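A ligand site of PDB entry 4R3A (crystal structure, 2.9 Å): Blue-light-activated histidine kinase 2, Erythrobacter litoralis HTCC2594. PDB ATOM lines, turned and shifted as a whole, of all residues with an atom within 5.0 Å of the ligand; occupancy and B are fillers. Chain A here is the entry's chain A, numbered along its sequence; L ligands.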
ATOM      1  N   THR A  27      20.127 -16.275  24.314  1.00  0.00           N
ATOM      2  CA  THR A  27      19.194 -17.009  23.480  1.00  0.00           C
ATOM      3  C   THR A  27      18.994 -16.308  22.157  1.00  0.00           C
ATOM      4  O   THR A  27      19.007 -15.071  22.085  1.00  0.00           O
ATOM      5  CB  THR A  27      17.827 -17.144  24.183  1.00  0.00           C
ATOM      6  OG1 THR A  27      17.241 -15.850  24.337  1.00  0.00           O
ATOM      7  CG2 THR A  27      17.983 -17.797  25.549  1.00  0.00           C
ATOM      8  N   ILE A  28      18.756 -17.090  21.119  1.00  0.00           N
ATOM      9  CA  ILE A  28      18.436 -16.569  19.798  1.00  0.00           C
ATOM     10  C   ILE A  28      17.191 -17.274  19.293  1.00  0.00           C
ATOM     11  O   ILE A  28      17.075 -18.491  19.357  1.00  0.00           O
ATOM     12  CB  ILE A  28      19.613 -16.777  18.833  1.00  0.00           C
ATOM     13  CG1 ILE A  28      20.752 -15.844  19.231  1.00  0.00           C
ATOM     14  CG2 ILE A  28      19.181 -16.509  17.394  1.00  0.00           C
ATOM     15  CD1 ILE A  28      22.046 -16.078  18.497  1.00  0.00           C
ATOM     16  N   ALA A  29      16.248 -16.467  18.801  1.00  0.00           N
ATOM     17  CA  ALA A  29      14.992 -16.979  18.251  1.00  0.00           C
ATOM     18  C   ALA A  29      14.817 -16.588  16.779  1.00  0.00           C
ATOM     19  O   ALA A  29      15.281 -15.528  16.349  1.00  0.00           O
ATOM     20  CB  ALA A  29      13.814 -16.470  19.072  1.00  0.00           C
ATOM     21  N   ILE A  31      12.081 -15.435  14.624  1.00  0.00           N
ATOM     22  CA  ILE A  31      10.709 -14.938  14.727  1.00  0.00           C
ATOM     23  C   ILE A  31       9.984 -15.016  13.385  1.00  0.00           C
ATOM     24  O   ILE A  31       8.820 -14.667  13.294  1.00  0.00           O
ATOM     25  CB  ILE A  31      10.640 -13.492  15.279  1.00  0.00           C
ATOM     26  CG1 ILE A  31      11.262 -12.486  14.313  1.00  0.00           C
ATOM     27  CG2 ILE A  31      11.308 -13.414  16.643  1.00  0.00           C
ATOM     28  CD1 ILE A  31      10.837 -11.062  14.617  1.00  0.00           C
ATOM     29  N   GLU A  36       7.677 -18.263  16.876  1.00  0.00           N
ATOM     30  CA  GLU A  36       8.961 -17.661  17.263  1.00  0.00           C
ATOM     31  C   GLU A  36       9.801 -18.575  18.157  1.00  0.00           C
ATOM     32  O   GLU A  36      10.113 -18.220  19.284  1.00  0.00           O
ATOM     33  CB  GLU A  36       8.730 -16.325  17.972  1.00  0.00           C
ATOM     34  CG  GLU A  36       8.144 -15.242  17.089  1.00  0.00           C
ATOM     35  CD  GLU A  36       6.690 -14.948  17.379  1.00  0.00           C
ATOM     36  OE1 GLU A  36       6.350 -14.695  18.558  1.00  0.00           O
ATOM     37  OE2 GLU A  36       5.886 -14.981  16.414  1.00  0.00           O
ATOM     38  N   LEU A  38      12.869 -20.728  19.821  1.00  0.00           N
ATOM     39  CA  LEU A  38      14.295 -20.641  20.124  1.00  0.00           C
ATOM     40  C   LEU A  38      15.054 -21.541  19.176  1.00  0.00           C
ATOM     41  O   LEU A  38      14.683 -22.700  18.987  1.00  0.00           O
ATOM     42  CB  LEU A  38      14.568 -21.040  21.576  1.00  0.00           C
ATOM     43  CG  LEU A  38      14.144 -20.028  22.628  1.00  0.00           C
ATOM     44  CD1 LEU A  38      14.159 -20.662  24.003  1.00  0.00           C
ATOM     45  CD2 LEU A  38      15.060 -18.834  22.588  1.00  0.00           C
ATOM     46  N   ASN A  60       8.841 -21.742  21.916  1.00  0.00           N
ATOM     47  CA  ASN A  60       8.850 -20.348  22.346  1.00  0.00           C
ATOM     48  C   ASN A  60       9.299 -20.196  23.789  1.00  0.00           C
ATOM     49  O   ASN A  60       8.879 -20.965  24.659  1.00  0.00           O
ATOM     50  CB  ASN A  60       7.481 -19.711  22.162  1.00  0.00           C
ATOM     51  CG  ASN A  60       7.509 -18.223  22.390  1.00  0.00           C
ATOM     52  OD1 ASN A  60       7.382 -17.748  23.521  1.00  0.00           O
ATOM     53  ND2 ASN A  60       7.684 -17.460  21.313  1.00  0.00           N
ATOM     54  N   CYS A  61      10.117 -19.194  24.062  1.00  0.00           N
ATOM     55  CA  CYS A  61      10.732 -19.033  25.370  1.00  0.00           C
ATOM     56  C   CYS A  61       9.718 -18.735  26.492  1.00  0.00           C
ATOM     57  O   CYS A  61      10.087 -18.725  27.677  1.00  0.00           O
ATOM     58  CB  CYS A  61      11.778 -17.918  25.309  1.00  0.00           C
ATOM     59  SG  CYS A  61      13.052 -18.056  26.578  1.00  0.00           S
ATOM     60  N   ARG A  62       8.454 -18.519  26.147  1.00  0.00           N
ATOM     61  CA  ARG A  62       7.442 -18.152  27.130  1.00  0.00           C
ATOM     62  C   ARG A  62       7.138 -19.252  28.148  1.00  0.00           C
ATOM     63  O   ARG A  62       6.373 -19.033  29.083  1.00  0.00           O
ATOM     64  CB  ARG A  62       6.138 -17.751  26.436  1.00  0.00           C
ATOM     65  CG  ARG A  62       5.400 -18.896  25.740  1.00  0.00           C
ATOM     66  CD  ARG A  62       4.005 -18.483  25.311  1.00  0.00           C
ATOM     67  NE  ARG A  62       4.016 -17.256  24.513  1.00  0.00           N
ATOM     68  CZ  ARG A  62       4.191 -17.208  23.193  1.00  0.00           C
ATOM     69  NH1 ARG A  62       4.369 -18.334  22.488  1.00  0.00           N
ATOM     70  NH2 ARG A  62       4.176 -16.033  22.571  1.00  0.00           N
ATOM     71  N   LEU A  64       9.047 -20.064  30.318  1.00  0.00           N
ATOM     72  CA  LEU A  64       9.626 -19.588  31.563  1.00  0.00           C
ATOM     73  C   LEU A  64       8.652 -18.770  32.406  1.00  0.00           C
ATOM     74  O   LEU A  64       8.913 -18.499  33.578  1.00  0.00           O
ATOM     75  CB  LEU A  64      10.865 -18.739  31.281  1.00  0.00           C
ATOM     76  CG  LEU A  64      12.039 -19.426  30.581  1.00  0.00           C
ATOM     77  CD1 LEU A  64      13.044 -18.394  30.103  1.00  0.00           C
ATOM     78  CD2 LEU A  64      12.705 -20.423  31.515  1.00  0.00           C
ATOM     79  N   GLN A  65       7.522 -18.378  31.820  1.00  0.00           N
ATOM     80  CA  GLN A  65       6.588 -17.500  32.506  1.00  0.00           C
ATOM     81  C   GLN A  65       5.590 -18.315  33.335  1.00  0.00           C
ATOM     82  O   GLN A  65       5.450 -19.524  33.127  1.00  0.00           O
ATOM     83  CB  GLN A  65       5.845 -16.628  31.487  1.00  0.00           C
ATOM     84  CG  GLN A  65       6.760 -15.751  30.648  1.00  0.00           C
ATOM     85  CD  GLN A  65       6.018 -15.033  29.527  1.00  0.00           C
ATOM     86  OE1 GLN A  65       4.793 -14.969  29.520  1.00  0.00           O
ATOM     87  NE2 GLN A  65       6.771 -14.489  28.575  1.00  0.00           N
ATOM     88  N   VAL A  74       4.838  -8.730  29.740  1.00  0.00           N
ATOM     89  CA  VAL A  74       4.709  -9.667  28.629  1.00  0.00           C
ATOM     90  C   VAL A  74       4.195  -9.010  27.366  1.00  0.00           C
ATOM     91  O   VAL A  74       4.693  -9.288  26.267  1.00  0.00           O
ATOM     92  CB  VAL A  74       3.765 -10.833  28.994  1.00  0.00           C
ATOM     93  CG1 VAL A  74       3.479 -11.711  27.765  1.00  0.00           C
ATOM     94  CG2 VAL A  74       4.382 -11.660  30.103  1.00  0.00           C
ATOM     95  N   LEU A  77       6.879  -7.062  25.746  1.00  0.00           N
ATOM     96  CA  LEU A  77       7.768  -7.925  24.988  1.00  0.00           C
ATOM     97  C   LEU A  77       7.119  -8.265  23.654  1.00  0.00           C
ATOM     98  O   LEU A  77       7.755  -8.186  22.602  1.00  0.00           O
ATOM     99  CB  LEU A  77       8.069  -9.211  25.761  1.00  0.00           C
ATOM    100  CG  LEU A  77       8.802  -9.092  27.094  1.00  0.00           C
ATOM    101  CD1 LEU A  77       9.061 -10.483  27.653  1.00  0.00           C
ATOM    102  CD2 LEU A  77      10.106  -8.332  26.926  1.00  0.00           C
ATOM    103  N   ALA A  78       5.826  -8.596  23.696  1.00  0.00           N
ATOM    104  CA  ALA A  78       5.092  -8.985  22.498  1.00  0.00           C
ATOM    105  C   ALA A  78       5.083  -7.835  21.494  1.00  0.00           C
ATOM    106  O   ALA A  78       5.254  -8.035  20.291  1.00  0.00           O
ATOM    107  CB  ALA A  78       3.677  -9.406  22.844  1.00  0.00           C
ATOM    108  N   ILE A  81       8.568  -7.368  19.818  1.00  0.00           N
ATOM    109  CA  ILE A  81       8.845  -8.309  18.748  1.00  0.00           C
ATOM    110  C   ILE A  81       8.121  -7.872  17.491  1.00  0.00           C
ATOM    111  O   ILE A  81       8.712  -7.831  16.415  1.00  0.00           O
ATOM    112  CB  ILE A  81       8.428  -9.727  19.134  1.00  0.00           C
ATOM    113  CG1 ILE A  81       9.232 -10.201  20.331  1.00  0.00           C
ATOM    114  CG2 ILE A  81       8.632 -10.671  17.956  1.00  0.00           C
ATOM    115  CD1 ILE A  81       8.754 -11.523  20.929  1.00  0.00           C
ATOM    116  N   ILE A  91      11.616  -9.297  34.664  1.00  0.00           N
ATOM    117  CA  ILE A  91      10.408 -10.125  34.644  1.00  0.00           C
ATOM    118  C   ILE A  91      10.534 -11.357  35.517  1.00  0.00           C
ATOM    119  O   ILE A  91      11.621 -11.937  35.618  1.00  0.00           O
ATOM    120  CB  ILE A  91      10.055 -10.548  33.204  1.00  0.00           C
ATOM    121  CG1 ILE A  91       8.733 -11.306  33.182  1.00  0.00           C
ATOM    122  CG2 ILE A  91      11.159 -11.393  32.610  1.00  0.00           C
ATOM    123  CD1 ILE A  91       8.104 -11.362  31.812  1.00  0.00           C
ATOM    124  N   ASN A  93      10.153 -15.141  36.358  1.00  0.00           N
ATOM    125  CA  ASN A  93      10.207 -16.349  35.540  1.00  0.00           C
ATOM    126  C   ASN A  93      10.302 -17.554  36.461  1.00  0.00           C
ATOM    127  O   ASN A  93      10.498 -17.404  37.659  1.00  0.00           O
ATOM    128  CB  ASN A  93      11.402 -16.327  34.577  1.00  0.00           C
ATOM    129  CG  ASN A  93      11.160 -15.518  33.301  1.00  0.00           C
ATOM    130  OD1 ASN A  93      12.082 -15.317  32.517  1.00  0.00           O
ATOM    131  ND2 ASN A  93       9.927 -15.050  33.078  1.00  0.00           N
ATOM    132  N   ASN A 103      14.082 -12.148  36.441  1.00  0.00           N
ATOM    133  CA  ASN A 103      14.939 -12.211  35.264  1.00  0.00           C
ATOM    134  C   ASN A 103      15.064 -10.863  34.584  1.00  0.00           C
ATOM    135  O   ASN A 103      14.071 -10.345  34.082  1.00  0.00           O
ATOM    136  CB  ASN A 103      14.396 -13.245  34.270  1.00  0.00           C
ATOM    137  CG  ASN A 103      15.189 -13.280  32.975  1.00  0.00           C
ATOM    138  OD1 ASN A 103      16.238 -12.642  32.849  1.00  0.00           O
ATOM    139  ND2 ASN A 103      14.678 -14.025  32.004  1.00  0.00           N
ATOM    140  N   LEU A 105      15.797  -9.136  31.550  1.00  0.00           N
ATOM    141  CA  LEU A 105      15.838  -9.513  30.147  1.00  0.00           C
ATOM    142  C   LEU A 105      16.121  -8.319  29.231  1.00  0.00           C
ATOM    143  O   LEU A 105      15.447  -7.302  29.332  1.00  0.00           O
ATOM    144  CB  LEU A 105      14.519 -10.167  29.783  1.00  0.00           C
ATOM    145  CG  LEU A 105      14.273 -10.663  28.368  1.00  0.00           C
ATOM    146  CD1 LEU A 105      15.358 -11.617  27.923  1.00  0.00           C
ATOM    147  CD2 LEU A 105      12.903 -11.337  28.310  1.00  0.00           C
ATOM    148  N   MET A 107      16.498  -7.632  25.114  1.00  0.00           N
ATOM    149  CA  MET A 107      16.364  -8.234  23.792  1.00  0.00           C
ATOM    150  C   MET A 107      15.982  -7.258  22.698  1.00  0.00           C
ATOM    151  O   MET A 107      15.543  -6.142  22.963  1.00  0.00           O
ATOM    152  CB  MET A 107      15.314  -9.347  23.834  1.00  0.00           C
ATOM    153  CG  MET A 107      13.927  -8.917  23.292  1.00  0.00           C
ATOM    154  SD  MET A 107      12.694 -10.219  23.327  1.00  0.00           S
ATOM    155  CE  MET A 107      12.669 -10.568  25.077  1.00  0.00           C
ATOM    156  N   PHE A 120      15.871 -12.707  16.556  1.00  0.00           N
ATOM    157  CA  PHE A 120      15.958 -11.979  17.804  1.00  0.00           C
ATOM    158  C   PHE A 120      16.923 -12.618  18.774  1.00  0.00           C
ATOM    159  O   PHE A 120      17.068 -13.834  18.816  1.00  0.00           O
ATOM    160  CB  PHE A 120      14.580 -11.910  18.462  1.00  0.00           C
ATOM    161  CG  PHE A 120      13.867 -10.604  18.284  1.00  0.00           C
ATOM    162  CD1 PHE A 120      13.362 -10.239  17.050  1.00  0.00           C
ATOM    163  CD2 PHE A 120      13.674  -9.754  19.361  1.00  0.00           C
ATOM    164  CE1 PHE A 120      12.686  -9.045  16.898  1.00  0.00           C
ATOM    165  CE2 PHE A 120      12.998  -8.560  19.209  1.00  0.00           C
ATOM    166  CZ  PHE A 120      12.505  -8.195  17.984  1.00  0.00           C
ATOM    167  N   VAL A 121      17.566 -11.759  19.541  1.00  0.00           N
ATOM    168  CA  VAL A 121      18.492 -12.152  20.587  1.00  0.00           C
ATOM    169  C   VAL A 121      18.017 -11.536  21.868  1.00  0.00           C
ATOM    170  O   VAL A 121      17.431 -10.451  21.854  1.00  0.00           O
ATOM    171  CB  VAL A 121      19.931 -11.666  20.312  1.00  0.00           C
ATOM    172  CG1 VAL A 121      19.960 -10.140  20.134  1.00  0.00           C
ATOM    173  CG2 VAL A 121      20.863 -12.074  21.437  1.00  0.00           C
ATOM    174  N   GLY A 122      18.213 -12.242  22.967  1.00  0.00           N
ATOM    175  CA  GLY A 122      17.770 -11.746  24.254  1.00  0.00           C
ATOM    176  C   GLY A 122      18.851 -12.193  25.203  1.00  0.00           C
ATOM    177  O   GLY A 122      19.411 -13.286  25.038  1.00  0.00           O
ATOM    178  N   GLN A 124      19.677 -12.840  29.420  1.00  0.00           N
ATOM    179  CA  GLN A 124      19.048 -13.006  30.710  1.00  0.00           C
ATOM    180  C   GLN A 124      20.058 -12.954  31.840  1.00  0.00           C
ATOM    181  O   GLN A 124      21.098 -13.591  31.752  1.00  0.00           O
ATOM    182  CB  GLN A 124      18.275 -14.329  30.744  1.00  0.00           C
ATOM    183  CG  GLN A 124      17.232 -14.473  29.644  1.00  0.00           C
ATOM    184  CD  GLN A 124      17.845 -14.855  28.300  1.00  0.00           C
ATOM    185  OE1 GLN A 124      18.694 -15.743  28.213  1.00  0.00           O
ATOM    186  NE2 GLN A 124      17.412 -14.181  27.237  1.00  0.00           N
HETATM  187  N1  LIG L   1      10.069 -14.067  28.159  1.00  0.00           N
HETATM  188  C1  LIG L   1      10.389 -14.315  29.448  1.00  0.00           C
HETATM  189  O1  LIG L   1       9.552 -14.202  30.318  1.00  0.00           O
HETATM  190  N2  LIG L   1      11.634 -14.681  29.788  1.00  0.00           N
HETATM  191  C2  LIG L   1      12.603 -14.792  28.861  1.00  0.00           C
HETATM  192  O2  LIG L   1      13.732 -15.117  29.186  1.00  0.00           O
HETATM  193  C3  LIG L   1      12.322 -14.510  27.516  1.00  0.00           C
HETATM  194  N3  LIG L   1      13.279 -14.579  26.584  1.00  0.00           N
HETATM  195  C4  LIG L   1      13.004 -14.293  25.320  1.00  0.00           C
HETATM  196  C5  LIG L   1      14.048 -14.381  24.359  1.00  0.00           C
HETATM  197  C6  LIG L   1      13.800 -14.100  23.027  1.00  0.00           C
HETATM  198  C7  LIG L   1      14.969 -14.216  22.030  1.00  0.00           C
HETATM  199  C8  LIG L   1      12.540 -13.719  22.610  1.00  0.00           C
HETATM  200  C9  LIG L   1      12.235 -13.399  21.149  1.00  0.00           C
HETATM  201  C10 LIG L   1      11.500 -13.629  23.539  1.00  0.00           C
HETATM  202  C11 LIG L   1      11.714 -13.912  24.908  1.00  0.00           C
HETATM  203  N4  LIG L   1      10.685 -13.822  25.835  1.00  0.00           N
HETATM  204  C12 LIG L   1      10.997 -14.124  27.183  1.00  0.00           C
HETATM  205  C13 LIG L   1       9.327 -13.425  25.490  1.00  0.00           C
HETATM  206  C14 LIG L   1       8.471 -14.641  25.118  1.00  0.00           C
HETATM  207  O3  LIG L   1       9.252 -15.625  24.528  1.00  0.00           O
HETATM  208  C15 LIG L   1       7.366 -14.232  24.150  1.00  0.00           C
HETATM  209  O4  LIG L   1       7.944 -13.861  22.926  1.00  0.00           O
HETATM  210  C16 LIG L   1       6.547 -13.086  24.709  1.00  0.00           C
HETATM  211  O5  LIG L   1       6.289 -13.317  26.063  1.00  0.00           O
HETATM  212  C17 LIG L   1       5.229 -12.971  23.937  1.00  0.00           C
HETATM  213  O6  LIG L   1       4.278 -13.884  24.433  1.00  0.00           O
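OD1 of Asn 93 is in hydrogen-bond range of ND2 of Asn 103.
The backbone NH (N) of Arg 62 sits at hydrogen-bond distance from the side-chain amide oxygen (OD1) of Asn 60, at 2.9 Å.
The side-chain amide nitrogen (ND2) of Asn 60 lies within hydrogen-bond range of the backbone carbonyl oxygen (O) of Glu 36 (3.3 Å).
The backbone NH of Asn 103 sits at hydrogen-bond distance from the backbone carbonyl oxygen of Ile 91, 2.6 Å away.
The side-chain hydroxyl (OG1) of Thr 27 lies within hydrogen-bond range of the side-chain amide nitrogen (NE2) of Gln 124 (3.4 Å).
The backbone carbonyl oxygen (O) of Thr 27 sits at hydrogen-bond distance from the backbone NH (N) of Gly 122, 3.1 Å away.
The side-chain amide nitrogen of Gln 124 is in hydrogen-bond range of the backbone carbonyl oxygen of Gly 122 (3.1 Å).
N of Ala 29 is in hydrogen-bond range of O of Phe 120.
The side-chain amide nitrogen (NE2) of Gln 65 is in hydrogen-bond range of an oxygen (O5) of the ligand.
The side-chain amide oxygen of Asn 93 lies within hydrogen-bond range of a nitrogen (N2) of the ligand, 2.8 Å away.
N of Arg 62 is in hydrogen-bond range of O3 of the ligand (3.4 Å).
NH2 of Arg 62 lies within hydrogen-bond range of O6 of the ligand.
An oxygen (O3) of the ligand is in hydrogen-bond range of the side-chain amide oxygen (OD1) of Asn 60 (3.0 Å).
The side-chain amide nitrogen (ND2) of Asn 103 is in hydrogen-bond range of an oxygen (O2) of the ligand.
The side-chain sulfur (SG) of Cys 61 sits at hydrogen-bond distance from a nitrogen (N3) of the ligand, 3.5 Å away.
Residues that only touch the ligand: Thr 27, Ala 29, Leu 64, Val 74, Leu 77, Ile 81, Ile 91, Leu 105, Met 107, Phe 120, Gly 122 and Gln 124.
Of the 24 residues printed, 18 come within 4 Å of the ligand.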
